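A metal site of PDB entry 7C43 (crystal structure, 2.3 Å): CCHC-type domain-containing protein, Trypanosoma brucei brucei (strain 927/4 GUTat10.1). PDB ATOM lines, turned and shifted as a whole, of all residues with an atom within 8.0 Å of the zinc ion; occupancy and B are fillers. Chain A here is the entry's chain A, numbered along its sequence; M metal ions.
The zinc ion is bound by SG of Cys 261 (2.1 Å), SG of Cys 271 (2.2 Å), NE2 of His 266 (2.3 Å) and SG of Cys 258 (2.4 Å).
The side-chain sulfur (SG) of Cys 258 lies close to the backbone NH (N) of Phe 260. The side-chain sulfur (SG) of Cys 271 lies close to the backbone NH (N) of Lys 273. N of Lys 274 sits close to SG of Cys 271 (3.7 Å). N of Glu 268 lies close to SG of Cys 258 (3.7 Å). The backbone carbonyl oxygen (O) of Ala 263 sits at hydrogen-bond distance from the backbone NH (N) of Cys 258 (2.8 Å). The side-chain sulfur of Cys 261 lies close to the backbone NH of Ala 263.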
ATOM      1  N   GLY A 257      -5.934 -28.433  28.122  1.00  0.00           N
ATOM      2  CA  GLY A 257      -6.307 -27.217  27.455  1.00  0.00           C
ATOM      3  C   GLY A 257      -5.257 -26.157  27.628  1.00  0.00           C
ATOM      4  O   GLY A 257      -4.164 -26.432  28.163  1.00  0.00           O
ATOM      5  N   CYS A 258      -5.617 -24.941  27.205  1.00  0.00           N
ATOM      6  CA  CYS A 258      -4.695 -23.835  27.176  1.00  0.00           C
ATOM      7  C   CYS A 258      -4.410 -23.308  28.583  1.00  0.00           C
ATOM      8  O   CYS A 258      -5.320 -22.849  29.316  1.00  0.00           O
ATOM      9  CB  CYS A 258      -5.219 -22.710  26.272  1.00  0.00           C
ATOM     10  SG  CYS A 258      -4.019 -21.382  26.001  1.00  0.00           S
ATOM     11  N   HIS A 259      -3.143 -23.386  28.954  1.00  0.00           N
ATOM     12  CA  HIS A 259      -2.633 -22.838  30.205  1.00  0.00           C
ATOM     13  C   HIS A 259      -2.701 -21.309  30.263  1.00  0.00           C
ATOM     14  O   HIS A 259      -2.744 -20.737  31.356  1.00  0.00           O
ATOM     15  CB  HIS A 259      -1.188 -23.311  30.477  1.00  0.00           C
ATOM     16  CG  HIS A 259      -1.064 -24.804  30.652  1.00  0.00           C
ATOM     17  ND1 HIS A 259       0.148 -25.447  30.805  1.00  0.00           N
ATOM     18  CD2 HIS A 259      -2.015 -25.786  30.676  1.00  0.00           C
ATOM     19  CE1 HIS A 259      -0.053 -26.748  30.914  1.00  0.00           C
ATOM     20  NE2 HIS A 259      -1.347 -26.982  30.843  1.00  0.00           N
ATOM     21  N   PHE A 260      -2.721 -20.643  29.120  1.00  0.00           N
ATOM     22  CA  PHE A 260      -2.807 -19.179  29.123  1.00  0.00           C
ATOM     23  C   PHE A 260      -4.239 -18.661  29.335  1.00  0.00           C
ATOM     24  O   PHE A 260      -4.465 -17.855  30.247  1.00  0.00           O
ATOM     25  CB  PHE A 260      -2.177 -18.590  27.883  1.00  0.00           C
ATOM     26  CG  PHE A 260      -2.004 -17.097  27.962  1.00  0.00           C
ATOM     27  CD1 PHE A 260      -0.918 -16.541  28.632  1.00  0.00           C
ATOM     28  CD2 PHE A 260      -2.964 -16.237  27.398  1.00  0.00           C
ATOM     29  CE1 PHE A 260      -0.773 -15.164  28.710  1.00  0.00           C
ATOM     30  CE2 PHE A 260      -2.822 -14.848  27.483  1.00  0.00           C
ATOM     31  CZ  PHE A 260      -1.720 -14.318  28.131  1.00  0.00           C
ATOM     32  N   CYS A 261      -5.211 -19.129  28.540  1.00  0.00           N
ATOM     33  CA  CYS A 261      -6.609 -18.639  28.606  1.00  0.00           C
ATOM     34  C   CYS A 261      -7.598 -19.585  29.245  1.00  0.00           C
ATOM     35  O   CYS A 261      -8.714 -19.173  29.506  1.00  0.00           O
ATOM     36  CB  CYS A 261      -7.146 -18.248  27.217  1.00  0.00           C
ATOM     37  SG  CYS A 261      -7.372 -19.600  26.057  1.00  0.00           S
ATOM     38  N   GLY A 262      -7.210 -20.833  29.495  1.00  0.00           N
ATOM     39  CA  GLY A 262      -8.080 -21.809  30.163  1.00  0.00           C
ATOM     40  C   GLY A 262      -8.989 -22.623  29.253  1.00  0.00           C
ATOM     41  O   GLY A 262      -9.597 -23.562  29.727  1.00  0.00           O
ATOM     42  N   ALA A 263      -9.098 -22.282  27.973  1.00  0.00           N
ATOM     43  CA  ALA A 263     -10.021 -22.968  27.056  1.00  0.00           C
ATOM     44  C   ALA A 263      -9.446 -24.276  26.494  1.00  0.00           C
ATOM     45  O   ALA A 263      -8.244 -24.405  26.239  1.00  0.00           O
ATOM     46  CB  ALA A 263     -10.424 -22.042  25.898  1.00  0.00           C
ATOM     47  N   LYS A 264     -10.340 -25.236  26.288  1.00  0.00           N
ATOM     48  CA  LYS A 264     -10.021 -26.471  25.622  1.00  0.00           C
ATOM     49  C   LYS A 264      -9.851 -26.245  24.109  1.00  0.00           C
ATOM     50  O   LYS A 264     -10.322 -25.254  23.547  1.00  0.00           O
ATOM     51  CB  LYS A 264     -11.104 -27.509  25.914  1.00  0.00           C
ATOM     52  CG  LYS A 264     -11.217 -27.902  27.381  1.00  0.00           C
ATOM     53  CD  LYS A 264     -12.368 -28.861  27.631  1.00  0.00           C
ATOM     54  CE  LYS A 264     -12.579 -29.137  29.114  1.00  0.00           C
ATOM     55  NZ  LYS A 264     -11.416 -29.842  29.717  1.00  0.00           N
ATOM     56  N   GLY A 265      -9.117 -27.156  23.474  1.00  0.00           N
ATOM     57  CA  GLY A 265      -8.965 -27.149  22.015  1.00  0.00           C
ATOM     58  C   GLY A 265      -7.637 -26.668  21.491  1.00  0.00           C
ATOM     59  O   GLY A 265      -7.331 -26.873  20.310  1.00  0.00           O
ATOM     60  N   HIS A 266      -6.825 -26.018  22.323  1.00  0.00           N
ATOM     61  CA  HIS A 266      -5.529 -25.550  21.863  1.00  0.00           C
ATOM     62  C   HIS A 266      -4.593 -25.425  23.021  1.00  0.00           C
ATOM     63  O   HIS A 266      -5.020 -25.416  24.147  1.00  0.00           O
ATOM     64  CB  HIS A 266      -5.627 -24.207  21.104  1.00  0.00           C
ATOM     65  CG  HIS A 266      -6.097 -23.061  21.953  1.00  0.00           C
ATOM     66  ND1 HIS A 266      -7.429 -22.731  22.065  1.00  0.00           N
ATOM     67  CD2 HIS A 266      -5.434 -22.176  22.713  1.00  0.00           C
ATOM     68  CE1 HIS A 266      -7.561 -21.689  22.864  1.00  0.00           C
ATOM     69  NE2 HIS A 266      -6.367 -21.331  23.275  1.00  0.00           N
ATOM     70  N   THR A 267      -3.299 -25.356  22.717  1.00  0.00           N
ATOM     71  CA  THR A 267      -2.281 -25.117  23.715  1.00  0.00           C
ATOM     72  C   THR A 267      -1.890 -23.662  23.641  1.00  0.00           C
ATOM     73  O   THR A 267      -2.231 -22.961  22.684  1.00  0.00           O
ATOM     74  CB  THR A 267      -1.028 -25.951  23.446  1.00  0.00           C
ATOM     75  OG1 THR A 267      -0.491 -25.589  22.180  1.00  0.00           O
ATOM     76  CG2 THR A 267      -1.385 -27.409  23.472  1.00  0.00           C
ATOM     77  N   GLU A 268      -1.131 -23.234  24.657  1.00  0.00           N
ATOM     78  CA  GLU A 268      -0.719 -21.844  24.747  1.00  0.00           C
ATOM     79  C   GLU A 268       0.196 -21.371  23.598  1.00  0.00           C
ATOM     80  O   GLU A 268       0.069 -20.216  23.180  1.00  0.00           O
ATOM     81  CB  GLU A 268      -0.139 -21.541  26.143  1.00  0.00           C
ATOM     82  CG  GLU A 268       1.220 -22.123  26.444  1.00  0.00           C
ATOM     83  CD  GLU A 268       1.646 -21.822  27.865  1.00  0.00           C
ATOM     84  OE1 GLU A 268       1.398 -22.661  28.744  1.00  0.00           O
ATOM     85  OE2 GLU A 268       2.224 -20.747  28.086  1.00  0.00           O
ATOM     86  N   ALA A 269       1.020 -22.256  23.045  1.00  0.00           N
ATOM     87  CA  ALA A 269       1.849 -21.935  21.866  1.00  0.00           C
ATOM     88  C   ALA A 269       1.004 -21.555  20.631  1.00  0.00           C
ATOM     89  O   ALA A 269       1.496 -20.875  19.734  1.00  0.00           O
ATOM     90  CB  ALA A 269       2.792 -23.086  21.525  1.00  0.00           C
ATOM     91  N   GLU A 270      -0.256 -22.007  20.599  1.00  0.00           N
ATOM     92  CA  GLU A 270      -1.227 -21.670  19.558  1.00  0.00           C
ATOM     93  C   GLU A 270      -2.272 -20.623  20.031  1.00  0.00           C
ATOM     94  O   GLU A 270      -3.209 -20.313  19.262  1.00  0.00           O
ATOM     95  CB  GLU A 270      -1.989 -22.944  19.112  1.00  0.00           C
ATOM     96  CG  GLU A 270      -1.180 -24.249  19.010  1.00  0.00           C
ATOM     97  CD  GLU A 270      -2.047 -25.506  18.978  1.00  0.00           C
ATOM     98  OE1 GLU A 270      -3.013 -25.648  19.736  1.00  0.00           O
ATOM     99  OE2 GLU A 270      -1.741 -26.413  18.196  1.00  0.00           O
ATOM    100  N   CYS A 271      -2.131 -20.104  21.260  1.00  0.00           N
ATOM    101  CA  CYS A 271      -3.104 -19.132  21.804  1.00  0.00           C
ATOM    102  C   CYS A 271      -3.007 -17.729  21.149  1.00  0.00           C
ATOM    103  O   CYS A 271      -1.978 -17.044  21.268  1.00  0.00           O
ATOM    104  CB  CYS A 271      -2.963 -18.985  23.323  1.00  0.00           C
ATOM    105  SG  CYS A 271      -4.396 -18.224  24.131  1.00  0.00           S
ATOM    106  N   PHE A 272      -4.088 -17.332  20.458  1.00  0.00           N
ATOM    107  CA  PHE A 272      -4.213 -15.988  19.892  1.00  0.00           C
ATOM    108  C   PHE A 272      -3.993 -14.976  20.998  1.00  0.00           C
ATOM    109  O   PHE A 272      -3.186 -14.100  20.839  1.00  0.00           O
ATOM    110  CB  PHE A 272      -5.618 -15.729  19.280  1.00  0.00           C
ATOM    111  CG  PHE A 272      -5.762 -16.174  17.839  1.00  0.00           C
ATOM    112  CD1 PHE A 272      -6.133 -17.497  17.537  1.00  0.00           C
ATOM    113  CD2 PHE A 272      -5.583 -15.264  16.782  1.00  0.00           C
ATOM    114  CE1 PHE A 272      -6.290 -17.902  16.208  1.00  0.00           C
ATOM    115  CE2 PHE A 272      -5.746 -15.676  15.447  1.00  0.00           C
ATOM    116  CZ  PHE A 272      -6.096 -16.990  15.170  1.00  0.00           C
ATOM    117  N   LYS A 273      -4.711 -15.121  22.099  1.00  0.00           N
ATOM    118  CA  LYS A 273      -4.646 -14.123  23.175  1.00  0.00           C
ATOM    119  C   LYS A 273      -3.264 -13.995  23.796  1.00  0.00           C
ATOM    120  O   LYS A 273      -2.890 -12.901  24.214  1.00  0.00           O
ATOM    121  CB  LYS A 273      -5.665 -14.436  24.277  1.00  0.00           C
ATOM    122  CG  LYS A 273      -7.097 -14.255  23.840  1.00  0.00           C
ATOM    123  CD  LYS A 273      -8.027 -15.110  24.682  1.00  0.00           C
ATOM    124  CE  LYS A 273      -9.470 -14.647  24.584  1.00  0.00           C
ATOM    125  NZ  LYS A 273     -10.266 -15.319  25.647  1.00  0.00           N
ATOM    126  N   LYS A 274      -2.507 -15.072  23.844  1.00  0.00           N
ATOM    127  CA  LYS A 274      -1.152 -14.969  24.357  1.00  0.00           C
ATOM    128  C   LYS A 274      -0.231 -14.183  23.439  1.00  0.00           C
ATOM    129  O   LYS A 274       0.500 -13.338  23.940  1.00  0.00           O
ATOM    130  CB  LYS A 274      -0.545 -16.331  24.651  1.00  0.00           C
ATOM    131  CG  LYS A 274       0.774 -16.209  25.376  1.00  0.00           C
ATOM    132  CD  LYS A 274       1.342 -17.546  25.752  1.00  0.00           C
ATOM    133  CE  LYS A 274       2.793 -17.409  26.129  1.00  0.00           C
ATOM    134  NZ  LYS A 274       3.228 -18.632  26.851  1.00  0.00           N
HETATM  135 ZN    ZN M   1      -5.588 -19.903  24.969  1.00  0.00          ZN
